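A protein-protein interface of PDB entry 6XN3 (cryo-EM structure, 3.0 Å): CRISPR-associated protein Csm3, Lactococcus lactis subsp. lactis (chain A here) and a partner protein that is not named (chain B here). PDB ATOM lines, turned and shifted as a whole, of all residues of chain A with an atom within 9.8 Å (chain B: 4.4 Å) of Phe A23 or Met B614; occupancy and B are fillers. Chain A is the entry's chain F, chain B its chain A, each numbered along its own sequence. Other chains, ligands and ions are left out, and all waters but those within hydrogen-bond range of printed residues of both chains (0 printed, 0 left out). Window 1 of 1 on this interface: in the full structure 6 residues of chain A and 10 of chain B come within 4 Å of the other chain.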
ATOM      1  N   GLY A  19       5.900 -21.655  13.432  1.00  0.00           N
ATOM      2  CA  GLY A  19       5.838 -20.815  12.265  1.00  0.00           C
ATOM      3  C   GLY A  19       5.003 -19.583  12.522  1.00  0.00           C
ATOM      4  O   GLY A  19       3.814 -19.682  12.828  1.00  0.00           O
ATOM      5  N   SER A  20       5.622 -18.419  12.417  1.00  0.00           N
ATOM      6  CA  SER A  20       4.861 -17.190  12.382  1.00  0.00           C
ATOM      7  C   SER A  20       4.413 -16.913  10.954  1.00  0.00           C
ATOM      8  O   SER A  20       4.899 -17.519   9.996  1.00  0.00           O
ATOM      9  CB  SER A  20       5.691 -16.022  12.910  1.00  0.00           C
ATOM     10  OG  SER A  20       6.703 -15.667  11.987  1.00  0.00           O
ATOM     11  N   SER A  21       3.465 -15.993  10.817  1.00  0.00           N
ATOM     12  CA  SER A  21       3.069 -15.533   9.496  1.00  0.00           C
ATOM     13  C   SER A  21       3.819 -14.281   9.067  1.00  0.00           C
ATOM     14  O   SER A  21       3.311 -13.533   8.228  1.00  0.00           O
ATOM     15  CB  SER A  21       1.563 -15.281   9.454  1.00  0.00           C
ATOM     16  OG  SER A  21       0.856 -16.507   9.372  1.00  0.00           O
ATOM     17  N   ASP A  22       4.992 -14.035   9.644  1.00  0.00           N
ATOM     18  CA  ASP A  22       5.850 -12.927   9.255  1.00  0.00           C
ATOM     19  C   ASP A  22       6.307 -13.093   7.817  1.00  0.00           C
ATOM     20  O   ASP A  22       6.557 -14.208   7.355  1.00  0.00           O
ATOM     21  CB  ASP A  22       7.060 -12.862  10.184  1.00  0.00           C
ATOM     22  CG  ASP A  22       6.686 -12.449  11.591  1.00  0.00           C
ATOM     23  OD1 ASP A  22       5.693 -11.709  11.748  1.00  0.00           O
ATOM     24  OD2 ASP A  22       7.376 -12.877  12.541  1.00  0.00           O
ATOM     25  N   PHE A  23       6.378 -11.980   7.101  1.00  0.00           N
ATOM     26  CA  PHE A  23       6.771 -12.041   5.704  1.00  0.00           C
ATOM     27  C   PHE A  23       8.259 -12.316   5.584  1.00  0.00           C
ATOM     28  O   PHE A  23       9.084 -11.689   6.252  1.00  0.00           O
ATOM     29  CB  PHE A  23       6.433 -10.741   4.993  1.00  0.00           C
ATOM     30  CG  PHE A  23       6.937 -10.686   3.587  1.00  0.00           C
ATOM     31  CD1 PHE A  23       6.445 -11.547   2.627  1.00  0.00           C
ATOM     32  CD2 PHE A  23       7.913  -9.776   3.228  1.00  0.00           C
ATOM     33  CE1 PHE A  23       6.910 -11.495   1.329  1.00  0.00           C
ATOM     34  CE2 PHE A  23       8.379  -9.722   1.932  1.00  0.00           C
ATOM     35  CZ  PHE A  23       7.871 -10.581   0.982  1.00  0.00           C
ATOM     36  N   SER A  24       8.594 -13.257   4.716  1.00  0.00           N
ATOM     37  CA  SER A  24       9.972 -13.644   4.474  1.00  0.00           C
ATOM     38  C   SER A  24      10.493 -12.869   3.275  1.00  0.00           C
ATOM     39  O   SER A  24       9.860 -12.861   2.217  1.00  0.00           O
ATOM     40  CB  SER A  24      10.070 -15.146   4.222  1.00  0.00           C
ATOM     41  OG  SER A  24       9.134 -15.556   3.240  1.00  0.00           O
ATOM     42  N   ALA A  25      11.643 -12.225   3.441  1.00  0.00           N
ATOM     43  CA  ALA A  25      12.307 -11.583   2.319  1.00  0.00           C
ATOM     44  C   ALA A  25      12.869 -12.637   1.370  1.00  0.00           C
ATOM     45  O   ALA A  25      12.915 -13.830   1.680  1.00  0.00           O
ATOM     46  CB  ALA A  25      13.419 -10.662   2.809  1.00  0.00           C
ATOM     47  N   ILE A  26      13.301 -12.184   0.194  1.00  0.00           N
ATOM     48  CA  ILE A  26      13.558 -13.115  -0.901  1.00  0.00           C
ATOM     49  C   ILE A  26      14.868 -13.872  -0.680  1.00  0.00           C
ATOM     50  O   ILE A  26      14.970 -15.069  -0.970  1.00  0.00           O
ATOM     51  CB  ILE A  26      13.507 -12.380  -2.255  1.00  0.00           C
ATOM     52  CG1 ILE A  26      13.706 -13.347  -3.406  1.00  0.00           C
ATOM     53  CG2 ILE A  26      14.512 -11.261  -2.351  1.00  0.00           C
ATOM     54  CD1 ILE A  26      13.072 -12.873  -4.642  1.00  0.00           C
ATOM     55  N   GLY A  27      15.869 -13.213  -0.116  1.00  0.00           N
ATOM     56  CA  GLY A  27      17.127 -13.892   0.098  1.00  0.00           C
ATOM     57  C   GLY A  27      17.317 -14.295   1.541  1.00  0.00           C
ATOM     58  O   GLY A  27      18.405 -14.712   1.941  1.00  0.00           O
ATOM     59  N   ALA A  28      16.252 -14.188   2.329  1.00  0.00           N
ATOM     60  CA  ALA A  28      16.380 -14.284   3.774  1.00  0.00           C
ATOM     61  C   ALA A  28      15.619 -15.472   4.334  1.00  0.00           C
ATOM     62  O   ALA A  28      15.118 -16.315   3.588  1.00  0.00           O
ATOM     63  CB  ALA A  28      15.898 -12.997   4.441  1.00  0.00           C
ATOM     64  N   VAL A  29      15.537 -15.532   5.662  1.00  0.00           N
ATOM     65  CA  VAL A  29      15.027 -16.713   6.334  1.00  0.00           C
ATOM     66  C   VAL A  29      13.521 -16.787   6.189  1.00  0.00           C
ATOM     67  O   VAL A  29      12.788 -15.912   6.663  1.00  0.00           O
ATOM     68  CB  VAL A  29      15.429 -16.691   7.812  1.00  0.00           C
ATOM     69  CG1 VAL A  29      14.935 -17.932   8.493  1.00  0.00           C
ATOM     70  CG2 VAL A  29      16.928 -16.560   7.946  1.00  0.00           C
ATOM     71  N   ALA A  30      13.053 -17.822   5.510  1.00  0.00           N
ATOM     72  CA  ALA A  30      11.671 -18.246   5.607  1.00  0.00           C
ATOM     73  C   ALA A  30      11.542 -19.181   6.798  1.00  0.00           C
ATOM     74  O   ALA A  30      12.504 -19.843   7.187  1.00  0.00           O
ATOM     75  CB  ALA A  30      11.212 -18.942   4.325  1.00  0.00           C
ATOM     76  N   SER A  31      10.337 -19.235   7.362  1.00  0.00           N
ATOM     77  CA  SER A  31       9.984 -19.973   8.576  1.00  0.00           C
ATOM     78  C   SER A  31      10.916 -19.646   9.739  1.00  0.00           C
ATOM     79  O   SER A  31      11.802 -20.446  10.060  1.00  0.00           O
ATOM     80  CB  SER A  31       9.980 -21.487   8.336  1.00  0.00           C
ATOM     81  OG  SER A  31      11.278 -21.975   8.052  1.00  0.00           O
ATOM     82  N   PRO A  32      10.775 -18.487  10.372  1.00  0.00           N
ATOM     83  CA  PRO A  32      11.570 -18.205  11.565  1.00  0.00           C
ATOM     84  C   PRO A  32      11.032 -18.972  12.759  1.00  0.00           C
ATOM     85  O   PRO A  32       9.889 -19.426  12.787  1.00  0.00           O
ATOM     86  CB  PRO A  32      11.405 -16.700  11.743  1.00  0.00           C
ATOM     87  CG  PRO A  32      10.062 -16.437  11.217  1.00  0.00           C
ATOM     88  CD  PRO A  32       9.823 -17.401  10.092  1.00  0.00           C
ATOM     89  N   ARG B 513       2.578 -16.153  -6.245  1.00  0.00           N
ATOM     90  CA  ARG B 513       2.061 -15.587  -5.010  1.00  0.00           C
ATOM     91  C   ARG B 513       0.793 -14.797  -5.287  1.00  0.00           C
ATOM     92  O   ARG B 513       0.504 -14.436  -6.427  1.00  0.00           O
ATOM     93  CB  ARG B 513       3.084 -14.683  -4.328  1.00  0.00           C
ATOM     94  CG  ARG B 513       4.363 -15.383  -3.958  1.00  0.00           C
ATOM     95  CD  ARG B 513       4.101 -16.505  -2.981  1.00  0.00           C
ATOM     96  NE  ARG B 513       5.301 -17.277  -2.688  1.00  0.00           N
ATOM     97  CZ  ARG B 513       6.208 -16.933  -1.783  1.00  0.00           C
ATOM     98  NH1 ARG B 513       6.058 -15.827  -1.072  1.00  0.00           N
ATOM     99  NH2 ARG B 513       7.269 -17.700  -1.592  1.00  0.00           N
ATOM    100  N   LEU B 514       0.044 -14.528  -4.223  1.00  0.00           N
ATOM    101  CA  LEU B 514      -1.230 -13.826  -4.285  1.00  0.00           C
ATOM    102  C   LEU B 514      -1.103 -12.515  -3.522  1.00  0.00           C
ATOM    103  O   LEU B 514      -0.897 -12.524  -2.304  1.00  0.00           O
ATOM    104  CB  LEU B 514      -2.330 -14.700  -3.690  1.00  0.00           C
ATOM    105  CG  LEU B 514      -3.789 -14.481  -4.047  1.00  0.00           C
ATOM    106  CD1 LEU B 514      -4.031 -14.760  -5.506  1.00  0.00           C
ATOM    107  CD2 LEU B 514      -4.620 -15.406  -3.195  1.00  0.00           C
ATOM    108  N   GLY B 515      -1.223 -11.393  -4.231  1.00  0.00           N
ATOM    109  CA  GLY B 515      -0.997 -10.097  -3.629  1.00  0.00           C
ATOM    110  C   GLY B 515      -2.269  -9.388  -3.231  1.00  0.00           C
ATOM    111  O   GLY B 515      -3.297  -9.476  -3.893  1.00  0.00           O
ATOM    112  N   TRP B 584      -0.050 -10.630  -7.507  1.00  0.00           N
ATOM    113  CA  TRP B 584       0.696  -9.557  -6.859  1.00  0.00           C
ATOM    114  C   TRP B 584       1.253  -8.568  -7.866  1.00  0.00           C
ATOM    115  O   TRP B 584       1.451  -7.393  -7.533  1.00  0.00           O
ATOM    116  CB  TRP B 584       1.813 -10.136  -5.988  1.00  0.00           C
ATOM    117  CG  TRP B 584       3.055 -10.518  -6.709  1.00  0.00           C
ATOM    118  CD1 TRP B 584       3.349 -11.733  -7.239  1.00  0.00           C
ATOM    119  CD2 TRP B 584       4.190  -9.688  -6.952  1.00  0.00           C
ATOM    120  NE1 TRP B 584       4.592 -11.708  -7.813  1.00  0.00           N
ATOM    121  CE2 TRP B 584       5.127 -10.460  -7.651  1.00  0.00           C
ATOM    122  CE3 TRP B 584       4.495  -8.359  -6.662  1.00  0.00           C
ATOM    123  CZ2 TRP B 584       6.346  -9.951  -8.059  1.00  0.00           C
ATOM    124  CZ3 TRP B 584       5.706  -7.859  -7.061  1.00  0.00           C
ATOM    125  CH2 TRP B 584       6.618  -8.651  -7.752  1.00  0.00           C
ATOM    126  N   GLY B 613       0.208  -6.466   0.646  1.00  0.00           N
ATOM    127  CA  GLY B 613       0.723  -7.679   1.232  1.00  0.00           C
ATOM    128  C   GLY B 613       0.862  -8.734   0.156  1.00  0.00           C
ATOM    129  O   GLY B 613       0.304  -8.611  -0.931  1.00  0.00           O
ATOM    130  N   MET B 614       1.639  -9.769   0.461  1.00  0.00           N
ATOM    131  CA  MET B 614       1.874 -10.815  -0.527  1.00  0.00           C
ATOM    132  C   MET B 614       1.917 -12.165   0.165  1.00  0.00           C
ATOM    133  O   MET B 614       2.677 -12.357   1.117  1.00  0.00           O
ATOM    134  CB  MET B 614       3.156 -10.543  -1.316  1.00  0.00           C
ATOM    135  CG  MET B 614       3.447 -11.547  -2.402  1.00  0.00           C
ATOM    136  SD  MET B 614       4.938 -11.173  -3.337  1.00  0.00           S
ATOM    137  CE  MET B 614       6.208 -11.552  -2.159  1.00  0.00           C
ATOM    138  N   PHE B 615       1.104 -13.097  -0.330  1.00  0.00           N
ATOM    139  CA  PHE B 615       0.863 -14.380   0.308  1.00  0.00           C
ATOM    140  C   PHE B 615       0.886 -15.452  -0.764  1.00  0.00           C
ATOM    141  O   PHE B 615       0.799 -15.158  -1.954  1.00  0.00           O
ATOM    142  CB  PHE B 615      -0.483 -14.402   1.051  1.00  0.00           C
ATOM    143  CG  PHE B 615      -0.683 -13.247   1.998  1.00  0.00           C
ATOM    144  CD1 PHE B 615      -1.249 -12.062   1.564  1.00  0.00           C
ATOM    145  CD2 PHE B 615      -0.301 -13.350   3.319  1.00  0.00           C
ATOM    146  CE1 PHE B 615      -1.420 -11.006   2.426  1.00  0.00           C
ATOM    147  CE2 PHE B 615      -0.476 -12.290   4.186  1.00  0.00           C
ATOM    148  CZ  PHE B 615      -1.037 -11.120   3.735  1.00  0.00           C
ATOM    149  N   PHE B 655       4.682  -5.210   1.652  1.00  0.00           N
ATOM    150  CA  PHE B 655       4.801  -6.606   2.069  1.00  0.00           C
ATOM    151  C   PHE B 655       5.157  -6.782   3.543  1.00  0.00           C
ATOM    152  O   PHE B 655       5.096  -7.902   4.055  1.00  0.00           O
ATOM    153  CB  PHE B 655       5.838  -7.348   1.219  1.00  0.00           C
ATOM    154  CG  PHE B 655       5.666  -7.184  -0.264  1.00  0.00           C
ATOM    155  CD1 PHE B 655       4.414  -7.161  -0.852  1.00  0.00           C
ATOM    156  CD2 PHE B 655       6.777  -7.035  -1.070  1.00  0.00           C
ATOM    157  CE1 PHE B 655       4.280  -7.006  -2.211  1.00  0.00           C
ATOM    158  CE2 PHE B 655       6.645  -6.880  -2.425  1.00  0.00           C
ATOM    159  CZ  PHE B 655       5.394  -6.862  -2.994  1.00  0.00           C
ATOM    160  N   ASP B 656       5.487  -5.705   4.248  1.00  0.00           N
ATOM    161  CA  ASP B 656       6.033  -5.806   5.593  1.00  0.00           C
ATOM    162  C   ASP B 656       5.921  -4.442   6.254  1.00  0.00           C
ATOM    163  O   ASP B 656       5.853  -3.413   5.581  1.00  0.00           O
ATOM    164  CB  ASP B 656       7.493  -6.271   5.571  1.00  0.00           C
ATOM    165  CG  ASP B 656       7.974  -6.762   6.922  1.00  0.00           C
ATOM    166  OD1 ASP B 656       7.160  -6.807   7.866  1.00  0.00           O
ATOM    167  OD2 ASP B 656       9.171  -7.096   7.043  1.00  0.00           O
ATOM    168  N   LEU B 752      11.514 -11.015  -7.711  1.00  0.00           N
ATOM    169  CA  LEU B 752      10.161 -11.546  -7.592  1.00  0.00           C
ATOM    170  C   LEU B 752       9.399 -11.429  -8.907  1.00  0.00           C
ATOM    171  O   LEU B 752       8.556 -12.275  -9.218  1.00  0.00           O
ATOM    172  CB  LEU B 752       9.409 -10.830  -6.473  1.00  0.00           C
ATOM    173  CG  LEU B 752       9.784 -11.137  -5.026  1.00  0.00           C
ATOM    174  CD1 LEU B 752       9.216 -10.082  -4.097  1.00  0.00           C
ATOM    175  CD2 LEU B 752       9.330 -12.512  -4.621  1.00  0.00           C
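Among the printed residues, pairs that only touch across the chains: Phe A23 with Met B614 (3.6 Å), Phe A23 with Phe B655 (3.3 Å) and Ile A26 with Leu B752 (3.7 Å).
Printed residues of chain B that touch a printed residue of chain A: Met B614, Phe B655 and Leu B752.
Hydrophobic or aromatic side chains of chain B that line the printed part of chain A: Met B614, Phe B655 and Leu B752.
Of the 14 printed residues of chain A, 2 touch a printed residue of chain B.
Hydrophobic or aromatic side chains of chain A that line the printed part of chain B: Phe A23 and Ile A26.
Phe A23 touches just these residues of chain B: Met B614 (3.6 Å) and Phe B655 (3.3 Å).
No residue of chain A comes within 4 Å of Gly B613.
No residue of chain A comes within 4 Å of Phe B615.
Of the printed residues of chain B, Ile A26 touches Leu B752 (3.7 Å).
Of the printed residues of chain A, Leu B752 touches Ile A26 (3.7 Å).
Gly B515 touches none of the printed residues of chain A.
The nearest printed residue of chain B that does not touch Ile A26 is Met B614 (7.3 Å).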
